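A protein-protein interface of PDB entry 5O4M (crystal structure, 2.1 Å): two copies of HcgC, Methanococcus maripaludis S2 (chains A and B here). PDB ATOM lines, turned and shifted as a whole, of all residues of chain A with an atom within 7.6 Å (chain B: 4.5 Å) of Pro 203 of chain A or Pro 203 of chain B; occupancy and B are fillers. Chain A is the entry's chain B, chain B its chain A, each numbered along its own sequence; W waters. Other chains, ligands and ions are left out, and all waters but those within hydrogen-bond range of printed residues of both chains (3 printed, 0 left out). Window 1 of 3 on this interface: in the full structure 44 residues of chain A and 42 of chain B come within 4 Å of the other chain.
Among the printed residues, pairs that only touch across the chains: Val 182 of chain A with Thr 201 of chain B (3.6 Å), Val 182 of chain A with Ile 202 of chain B (3.6 Å), Met 186 of chain A with Met 186 of chain B (3.6 Å), Met 186 of chain A with Cys 189 of chain B (3.7 Å), Met 186 of chain A with Pro 203 of chain B (3.7 Å), Cys 189 of chain A with Met 186 of chain B (3.6 Å), Pro 203 of chain A with Met 186 of chain B (3.6 Å), Pro 203 of chain A with Pro 203 of chain B (3.9 Å), Asn 204 of chain A with Leu 205 of chain B (3.9 Å), Leu 205 of chain A with Asn 204 of chain B (3.9 Å), Lys 206 of chain A with Ile 202 of chain B (3.5 Å), Lys 206 of chain A with Asn 204 of chain B (3.8 Å) and Tyr 207 of chain A with Ile 202 of chain B (3.9 Å).
Water W2 bridges the side-chain amide oxygen (OD1) of Asn 204 of chain B (2.6 Å) and the backbone NH (N) of Tyr 207 of chain A (3.1 Å).
Water W1 bridges O of Leu 205 of chain B (2.8 Å) and O of Leu 205 of chain A (3.2 Å).
Water W3 lies within hydrogen-bond range of O of Leu 205 of chain A (3.1 Å) and OD1 of Asn 204 of chain B (3.3 Å).
The backbone carbonyl oxygen of Ile 185 of chain B sits at hydrogen-bond distance from the side-chain sulfur of Cys 189 of chain B (3.3 Å).
O of Ala 229 of chain B sits at hydrogen-bond distance from N of Asn 204 of chain B, 2.9 Å away.
SG of Cys 189 of chain A lies within hydrogen-bond range of O of Ile 185 of chain A (3.4 Å).
The side-chain amide nitrogen of Asn 204 of chain A is in hydrogen-bond range of the backbone carbonyl oxygen of Ser 228 of chain A.
N of Asn 204 of chain A sits at hydrogen-bond distance from O of Ala 229 of chain A (2.9 Å).
ND2 of Asn 204 of chain A lies within hydrogen-bond range of OG1 of Thr 231 of chain A (3.0 Å).
Printed residues of chain B that touch a printed residue of chain A: Met 186, Cys 189, Thr 201, Ile 202, Pro 203, Asn 204 and Leu 205.
Hydrophobic or aromatic side chains of chain B that line the printed part of chain A: Met 186, Ile 202, Pro 203 and Leu 205.
Among the printed residues, no Asp or Glu carboxylate lies within 4 Å of a Lys or Arg side-chain nitrogen of the other chain.
Met 186 of chain B touches its own counterpart, Met 186 of chain A.
Met 186 of chain A touches Cys 189 of chain B, and with the chains exchanged Cys 189 of chain A touches Met 186 of chain B.
Met 186 of chain A touches Pro 203 of chain B, and with the chains exchanged Pro 203 of chain A touches Met 186 of chain B.
Pro 203 of chain A touches Leu 205 of chain B, and with the chains exchanged Leu 205 of chain A touches Pro 203 of chain B.
Positions printed for both chains: 185, 186, 189, 201, 202, 203, 204, 205, 229 and 230.
Of the 16 pairs that touch across the chains among the printed residues, 11 have their exchanged pair printed and touching as well.
Pro 203 of chain A touches three residues of chain B.
Of the printed residues of chain A, Pro 203 of chain B touches Met 186, Pro 203 and Leu 205.
Of the printed residues of chain B, Val 182 of chain A touches Thr 201 and Ile 202.
Printed residues of chain A within 4 Å of Asn 204 of chain B: Leu 205 and Lys 206.
Of the printed residues of chain A, Cys 189 of chain B touches Met 186.
Ile 185 of chain A touches none of the printed residues of chain B.
The nearest residue of chain A that does not touch Pro 203 of chain B is Lys 206 of chain A (4.7 Å).
The backbone carbonyl oxygen (O) of Leu 205 of chain B lies close to the backbone carbonyl oxygen (O) of Pro 203 of chain A (3.4 Å).
O of Leu 205 of chain A sits close to O of Pro 203 of chain B (3.5 Å).
The backbone carbonyl oxygen of Leu 205 of chain A lies close to the backbone carbonyl oxygen of Leu 205 of chain B (3.3 Å).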
ATOM      1  N   ILE A  18       9.947  25.736  18.212  1.00  0.00           N
ATOM      2  CA  ILE A  18       9.628  24.309  18.282  1.00  0.00           C
ATOM      3  C   ILE A  18      10.872  23.497  17.835  1.00  0.00           C
ATOM      4  O   ILE A  18      11.156  22.452  18.427  1.00  0.00           O
ATOM      5  CB  ILE A  18       8.392  23.938  17.429  1.00  0.00           C
ATOM      6  CG1 ILE A  18       7.142  24.711  17.910  1.00  0.00           C
ATOM      7  CG2 ILE A  18       8.101  22.431  17.496  1.00  0.00           C
ATOM      8  CD1 ILE A  18       6.287  25.085  16.840  1.00  0.00           C
ATOM      9  N   VAL A 182       5.482  18.093  22.195  1.00  0.00           N
ATOM     10  CA  VAL A 182       4.122  18.498  22.419  1.00  0.00           C
ATOM     11  C   VAL A 182       3.850  18.580  23.922  1.00  0.00           C
ATOM     12  O   VAL A 182       3.316  19.583  24.393  1.00  0.00           O
ATOM     13  CB  VAL A 182       3.134  17.546  21.701  1.00  0.00           C
ATOM     14  CG1 VAL A 182       1.698  17.763  22.177  1.00  0.00           C
ATOM     15  CG2 VAL A 182       3.232  17.689  20.172  1.00  0.00           C
ATOM     16  N   ILE A 185       5.559  21.506  25.582  1.00  0.00           N
ATOM     17  CA  ILE A 185       4.876  22.745  25.212  1.00  0.00           C
ATOM     18  C   ILE A 185       3.596  22.927  25.995  1.00  0.00           C
ATOM     19  O   ILE A 185       3.363  24.004  26.519  1.00  0.00           O
ATOM     20  CB  ILE A 185       4.676  22.882  23.685  1.00  0.00           C
ATOM     21  CG1 ILE A 185       6.046  23.082  23.013  1.00  0.00           C
ATOM     22  CG2 ILE A 185       3.758  24.076  23.355  1.00  0.00           C
ATOM     23  CD1 ILE A 185       6.045  22.914  21.502  1.00  0.00           C
ATOM     24  N   MET A 186       2.794  21.885  26.069  1.00  0.00           N
ATOM     25  CA  MET A 186       1.523  21.895  26.787  1.00  0.00           C
ATOM     26  C   MET A 186       1.709  22.122  28.263  1.00  0.00           C
ATOM     27  O   MET A 186       0.950  22.879  28.849  1.00  0.00           O
ATOM     28  CB  MET A 186       0.786  20.563  26.563  1.00  0.00           C
ATOM     29  CG  MET A 186       0.277  20.386  25.131  1.00  0.00           C
ATOM     30  SD  MET A 186      -0.985  21.578  24.641  1.00  0.00           S
ATOM     31  CE  MET A 186      -2.392  20.978  25.546  1.00  0.00           C
ATOM     32  N   ASP A 187       2.692  21.487  28.876  1.00  0.00           N
ATOM     33  CA  ASP A 187       2.941  21.658  30.307  1.00  0.00           C
ATOM     34  C   ASP A 187       3.472  23.020  30.577  1.00  0.00           C
ATOM     35  O   ASP A 187       3.133  23.591  31.597  1.00  0.00           O
ATOM     36  CB  ASP A 187       3.846  20.574  30.872  1.00  0.00           C
ATOM     37  CG  ASP A 187       3.163  19.244  31.135  1.00  0.00           C
ATOM     38  OD1 ASP A 187       1.915  19.188  31.069  1.00  0.00           O
ATOM     39  OD2 ASP A 187       3.879  18.259  31.417  1.00  0.00           O
ATOM     40  N   CYS A 189       2.678  25.725  28.920  1.00  0.00           N
ATOM     41  CA  CYS A 189       1.480  26.589  28.779  1.00  0.00           C
ATOM     42  C   CYS A 189       0.629  26.654  30.012  1.00  0.00           C
ATOM     43  O   CYS A 189       0.060  27.679  30.313  1.00  0.00           O
ATOM     44  CB  CYS A 189       0.613  26.107  27.623  1.00  0.00           C
ATOM     45  SG  CYS A 189       1.196  26.633  26.032  1.00  0.00           S
ATOM     46  N   THR A 201      -2.609  31.861  26.889  1.00  0.00           N
ATOM     47  CA  THR A 201      -1.378  31.277  26.390  1.00  0.00           C
ATOM     48  C   THR A 201      -1.646  30.347  25.243  1.00  0.00           C
ATOM     49  O   THR A 201      -2.447  29.435  25.357  1.00  0.00           O
ATOM     50  CB  THR A 201      -0.684  30.549  27.526  1.00  0.00           C
ATOM     51  OG1 THR A 201      -0.629  31.424  28.652  1.00  0.00           O
ATOM     52  CG2 THR A 201       0.717  30.129  27.163  1.00  0.00           C
ATOM     53  N   ILE A 202      -0.957  30.574  24.135  1.00  0.00           N
ATOM     54  CA  ILE A 202      -1.121  29.780  22.933  1.00  0.00           C
ATOM     55  C   ILE A 202       0.051  28.850  22.656  1.00  0.00           C
ATOM     56  O   ILE A 202       1.142  29.323  22.404  1.00  0.00           O
ATOM     57  CB  ILE A 202      -1.233  30.721  21.700  1.00  0.00           C
ATOM     58  CG1 ILE A 202      -2.473  31.616  21.737  1.00  0.00           C
ATOM     59  CG2 ILE A 202      -1.148  29.955  20.359  1.00  0.00           C
ATOM     60  CD1 ILE A 202      -3.827  30.918  21.535  1.00  0.00           C
ATOM     61  N   PRO A 203      -0.156  27.539  22.626  1.00  0.00           N
ATOM     62  CA  PRO A 203       0.920  26.647  22.230  1.00  0.00           C
ATOM     63  C   PRO A 203       0.830  26.672  20.669  1.00  0.00           C
ATOM     64  O   PRO A 203      -0.258  26.411  20.120  1.00  0.00           O
ATOM     65  CB  PRO A 203       0.462  25.289  22.745  1.00  0.00           C
ATOM     66  CG  PRO A 203      -1.003  25.373  22.806  1.00  0.00           C
ATOM     67  CD  PRO A 203      -1.415  26.798  22.869  1.00  0.00           C
ATOM     68  N   ASN A 204       1.904  26.994  19.946  1.00  0.00           N
ATOM     69  CA  ASN A 204       1.835  27.035  18.468  1.00  0.00           C
ATOM     70  C   ASN A 204       2.006  25.641  17.924  1.00  0.00           C
ATOM     71  O   ASN A 204       3.067  25.278  17.416  1.00  0.00           O
ATOM     72  CB  ASN A 204       2.878  28.003  17.890  1.00  0.00           C
ATOM     73  CG  ASN A 204       2.566  29.436  18.249  1.00  0.00           C
ATOM     74  OD1 ASN A 204       1.467  29.925  17.980  1.00  0.00           O
ATOM     75  ND2 ASN A 204       3.463  30.119  18.943  1.00  0.00           N
ATOM     76  N   LEU A 205       0.943  24.835  18.041  1.00  0.00           N
ATOM     77  CA  LEU A 205       0.971  23.463  17.595  1.00  0.00           C
ATOM     78  C   LEU A 205       0.030  23.184  16.475  1.00  0.00           C
ATOM     79  O   LEU A 205      -0.936  23.897  16.259  1.00  0.00           O
ATOM     80  CB  LEU A 205       0.636  22.560  18.789  1.00  0.00           C
ATOM     81  CG  LEU A 205       1.629  22.588  19.942  1.00  0.00           C
ATOM     82  CD1 LEU A 205       1.078  21.848  21.146  1.00  0.00           C
ATOM     83  CD2 LEU A 205       2.974  22.021  19.522  1.00  0.00           C
ATOM     84  N   LYS A 206       0.341  22.109  15.770  1.00  0.00           N
ATOM     85  CA  LYS A 206      -0.433  21.592  14.642  1.00  0.00           C
ATOM     86  C   LYS A 206       0.013  20.152  14.453  1.00  0.00           C
ATOM     87  O   LYS A 206       0.963  19.690  15.093  1.00  0.00           O
ATOM     88  CB  LYS A 206      -0.207  22.405  13.344  1.00  0.00           C
ATOM     89  CG  LYS A 206       1.186  22.284  12.717  1.00  0.00           C
ATOM     90  CD  LYS A 206       1.186  22.872  11.299  1.00  0.00           C
ATOM     91  CE  LYS A 206       0.619  21.898  10.275  1.00  0.00           C
ATOM     92  NZ  LYS A 206       0.333  22.550   8.964  1.00  0.00           N
ATOM     93  N   TYR A 207      -0.655  19.456  13.578  1.00  0.00           N
ATOM     94  CA  TYR A 207      -0.342  18.064  13.272  1.00  0.00           C
ATOM     95  C   TYR A 207       0.813  18.056  12.275  1.00  0.00           C
ATOM     96  O   TYR A 207       0.643  17.837  11.083  1.00  0.00           O
ATOM     97  CB  TYR A 207      -1.592  17.354  12.779  1.00  0.00           C
ATOM     98  CG  TYR A 207      -1.388  15.913  12.410  1.00  0.00           C
ATOM     99  CD1 TYR A 207      -0.822  15.015  13.301  1.00  0.00           C
ATOM    100  CD2 TYR A 207      -1.799  15.429  11.170  1.00  0.00           C
ATOM    101  CE1 TYR A 207      -0.650  13.680  12.966  1.00  0.00           C
ATOM    102  CE2 TYR A 207      -1.625  14.101  10.821  1.00  0.00           C
ATOM    103  CZ  TYR A 207      -1.047  13.226  11.718  1.00  0.00           C
ATOM    104  OH  TYR A 207      -0.897  11.906  11.343  1.00  0.00           O
ATOM    105  N   MET A 227       8.601  28.229  14.054  1.00  0.00           N
ATOM    106  CA  MET A 227       7.669  29.033  14.809  1.00  0.00           C
ATOM    107  C   MET A 227       8.044  28.992  16.296  1.00  0.00           C
ATOM    108  O   MET A 227       8.597  27.990  16.778  1.00  0.00           O
ATOM    109  CB  MET A 227       6.243  28.457  14.592  1.00  0.00           C
ATOM    110  CG  MET A 227       5.103  29.310  15.126  1.00  0.00           C
ATOM    111  SD  MET A 227       4.846  30.826  14.179  1.00  0.00           S
ATOM    112  CE  MET A 227       4.915  32.094  15.529  1.00  0.00           C
ATOM    113  N   SER A 228       7.733  30.092  17.011  1.00  0.00           N
ATOM    114  CA  SER A 228       7.959  30.218  18.446  1.00  0.00           C
ATOM    115  C   SER A 228       7.101  29.128  19.040  1.00  0.00           C
ATOM    116  O   SER A 228       5.993  28.898  18.528  1.00  0.00           O
ATOM    117  CB  SER A 228       7.443  31.562  18.965  1.00  0.00           C
ATOM    118  OG  SER A 228       8.353  32.562  18.598  1.00  0.00           O
ATOM    119  N   ALA A 229       7.571  28.462  20.096  1.00  0.00           N
ATOM    120  CA  ALA A 229       6.787  27.404  20.720  1.00  0.00           C
ATOM    121  C   ALA A 229       5.514  27.941  21.377  1.00  0.00           C
ATOM    122  O   ALA A 229       4.461  27.279  21.316  1.00  0.00           O
ATOM    123  CB  ALA A 229       7.628  26.664  21.750  1.00  0.00           C
ATOM    124  N   ILE A 230       5.600  29.122  22.005  1.00  0.00           N
ATOM    125  CA  ILE A 230       4.464  29.721  22.691  1.00  0.00           C
ATOM    126  C   ILE A 230       4.326  31.198  22.438  1.00  0.00           C
ATOM    127  O   ILE A 230       5.313  31.901  22.296  1.00  0.00           O
ATOM    128  CB  ILE A 230       4.607  29.439  24.243  1.00  0.00           C
ATOM    129  CG1 ILE A 230       4.496  27.933  24.540  1.00  0.00           C
ATOM    130  CG2 ILE A 230       3.562  30.232  25.099  1.00  0.00           C
ATOM    131  CD1 ILE A 230       4.899  27.516  25.900  1.00  0.00           C
ATOM    132  N   THR A 231       3.079  31.662  22.405  1.00  0.00           N
ATOM    133  CA  THR A 231       2.709  33.049  22.228  1.00  0.00           C
ATOM    134  C   THR A 231       1.799  33.363  23.410  1.00  0.00           C
ATOM    135  O   THR A 231       0.854  32.634  23.667  1.00  0.00           O
ATOM    136  CB  THR A 231       2.081  33.328  20.868  1.00  0.00           C
ATOM    137  OG1 THR A 231       3.027  32.924  19.878  1.00  0.00           O
ATOM    138  CG2 THR A 231       1.739  34.823  20.688  1.00  0.00           C
ATOM    139  N   VAL A 232       2.094  34.431  24.135  1.00  0.00           N
ATOM    140  CA  VAL A 232       1.323  34.836  25.303  1.00  0.00           C
ATOM    141  C   VAL A 232       0.779  36.243  25.184  1.00  0.00           C
ATOM    142  O   VAL A 232       1.475  37.118  24.701  1.00  0.00           O
ATOM    143  CB  VAL A 232       2.222  34.826  26.564  1.00  0.00           C
ATOM    144  CG1 VAL A 232       1.375  34.915  27.826  1.00  0.00           C
ATOM    145  CG2 VAL A 232       3.130  33.604  26.602  1.00  0.00           C
ATOM    146  N   ILE B 185     -10.232  24.470  24.640  1.00  0.00           N
ATOM    147  CA  ILE B 185      -9.407  23.578  23.822  1.00  0.00           C
ATOM    148  C   ILE B 185      -8.290  22.935  24.629  1.00  0.00           C
ATOM    149  O   ILE B 185      -8.092  21.726  24.549  1.00  0.00           O
ATOM    150  CB  ILE B 185      -8.895  24.246  22.543  1.00  0.00           C
ATOM    151  CG1 ILE B 185     -10.075  24.528  21.606  1.00  0.00           C
ATOM    152  CG2 ILE B 185      -7.871  23.354  21.828  1.00  0.00           C
ATOM    153  CD1 ILE B 185      -9.788  25.470  20.476  1.00  0.00           C
ATOM    154  N   MET B 186      -7.591  23.732  25.402  1.00  0.00           N
ATOM    155  CA  MET B 186      -6.487  23.276  26.248  1.00  0.00           C
ATOM    156  C   MET B 186      -6.963  22.300  27.320  1.00  0.00           C
ATOM    157  O   MET B 186      -6.299  21.305  27.569  1.00  0.00           O
ATOM    158  CB  MET B 186      -5.806  24.467  26.919  1.00  0.00           C
ATOM    159  CG  MET B 186      -5.032  25.336  25.956  1.00  0.00           C
ATOM    160  SD  MET B 186      -3.613  24.567  25.117  1.00  0.00           S
ATOM    161  CE  MET B 186      -2.451  24.495  26.472  1.00  0.00           C
ATOM    162  N   CYS B 189      -7.886  19.027  25.700  1.00  0.00           N
ATOM    163  CA  CYS B 189      -6.635  18.343  25.323  1.00  0.00           C
ATOM    164  C   CYS B 189      -6.026  17.535  26.367  1.00  0.00           C
ATOM    165  O   CYS B 189      -5.549  16.438  26.059  1.00  0.00           O
ATOM    166  CB  CYS B 189      -5.611  19.324  24.788  1.00  0.00           C
ATOM    167  SG  CYS B 189      -5.919  19.743  23.097  1.00  0.00           S
ATOM    168  N   THR B 201      -1.897  14.527  21.818  1.00  0.00           N
ATOM    169  CA  THR B 201      -3.026  15.358  21.464  1.00  0.00           C
ATOM    170  C   THR B 201      -2.565  16.745  21.050  1.00  0.00           C
ATOM    171  O   THR B 201      -1.833  17.408  21.763  1.00  0.00           O
ATOM    172  CB  THR B 201      -3.976  15.423  22.643  1.00  0.00           C
ATOM    173  OG1 THR B 201      -4.220  14.097  23.104  1.00  0.00           O
ATOM    174  CG2 THR B 201      -5.294  16.043  22.281  1.00  0.00           C
ATOM    175  N   ILE B 202      -3.002  17.174  19.898  1.00  0.00           N
ATOM    176  CA  ILE B 202      -2.652  18.475  19.367  1.00  0.00           C
ATOM    177  C   ILE B 202      -3.785  19.467  19.416  1.00  0.00           C
ATOM    178  O   ILE B 202      -4.779  19.264  18.734  1.00  0.00           O
ATOM    179  CB  ILE B 202      -2.244  18.342  17.859  1.00  0.00           C
ATOM    180  CG1 ILE B 202      -0.995  17.494  17.654  1.00  0.00           C
ATOM    181  CG2 ILE B 202      -2.105  19.713  17.169  1.00  0.00           C
ATOM    182  CD1 ILE B 202       0.350  18.120  18.134  1.00  0.00           C
ATOM    183  N   PRO B 203      -3.655  20.572  20.161  1.00  0.00           N
ATOM    184  CA  PRO B 203      -4.702  21.610  20.103  1.00  0.00           C
ATOM    185  C   PRO B 203      -4.298  22.414  18.844  1.00  0.00           C
ATOM    186  O   PRO B 203      -3.139  22.876  18.774  1.00  0.00           O
ATOM    187  CB  PRO B 203      -4.453  22.435  21.346  1.00  0.00           C
ATOM    188  CG  PRO B 203      -3.006  22.247  21.652  1.00  0.00           C
ATOM    189  CD  PRO B 203      -2.518  20.998  20.989  1.00  0.00           C
ATOM    190  N   ASN B 204      -5.194  22.601  17.850  1.00  0.00           N
ATOM    191  CA  ASN B 204      -4.825  23.355  16.639  1.00  0.00           C
ATOM    192  C   ASN B 204      -4.966  24.824  16.930  1.00  0.00           C
ATOM    193  O   ASN B 204      -5.928  25.475  16.513  1.00  0.00           O
ATOM    194  CB  ASN B 204      -5.661  22.916  15.433  1.00  0.00           C
ATOM    195  CG  ASN B 204      -5.352  21.513  15.008  1.00  0.00           C
ATOM    196  OD1 ASN B 204      -4.196  21.186  14.746  1.00  0.00           O
ATOM    197  ND2 ASN B 204      -6.326  20.622  15.025  1.00  0.00           N
ATOM    198  N   LEU B 205      -3.995  25.364  17.651  1.00  0.00           N
ATOM    199  CA  LEU B 205      -4.007  26.764  18.031  1.00  0.00           C
ATOM    200  C   LEU B 205      -2.852  27.530  17.462  1.00  0.00           C
ATOM    201  O   LEU B 205      -1.808  26.985  17.124  1.00  0.00           O
ATOM    202  CB  LEU B 205      -3.959  26.868  19.563  1.00  0.00           C
ATOM    203  CG  LEU B 205      -5.167  26.289  20.283  1.00  0.00           C
ATOM    204  CD1 LEU B 205      -4.929  26.251  21.763  1.00  0.00           C
ATOM    205  CD2 LEU B 205      -6.438  27.086  19.957  1.00  0.00           C
ATOM    206  N   ALA B 229     -10.664  21.604  16.063  1.00  0.00           N
ATOM    207  CA  ALA B 229     -10.087  22.133  17.280  1.00  0.00           C
ATOM    208  C   ALA B 229      -8.943  21.250  17.781  1.00  0.00           C
ATOM    209  O   ALA B 229      -7.942  21.767  18.315  1.00  0.00           O
ATOM    210  CB  ALA B 229     -11.148  22.256  18.345  1.00  0.00           C
ATOM    211  N   ILE B 230      -9.081  19.924  17.620  1.00  0.00           N
ATOM    212  CA  ILE B 230      -8.073  18.980  18.099  1.00  0.00           C
ATOM    213  C   ILE B 230      -7.803  17.859  17.134  1.00  0.00           C
ATOM    214  O   ILE B 230      -8.697  17.404  16.440  1.00  0.00           O
ATOM    215  CB  ILE B 230      -8.544  18.403  19.490  1.00  0.00           C
ATOM    216  CG1 ILE B 230      -8.586  19.511  20.572  1.00  0.00           C
ATOM    217  CG2 ILE B 230      -7.652  17.223  19.973  1.00  0.00           C
ATOM    218  CD1 ILE B 230      -9.286  19.173  21.834  1.00  0.00           C
HETATM  219  O   HOH W   1       0.049  26.706  15.097  1.00  0.00           O
HETATM  220  O   HOH W   2      -3.328  20.386  12.408  1.00  0.00           O
HETATM  221  O   HOH W   3      -2.981  24.175  14.012  1.00  0.00           O
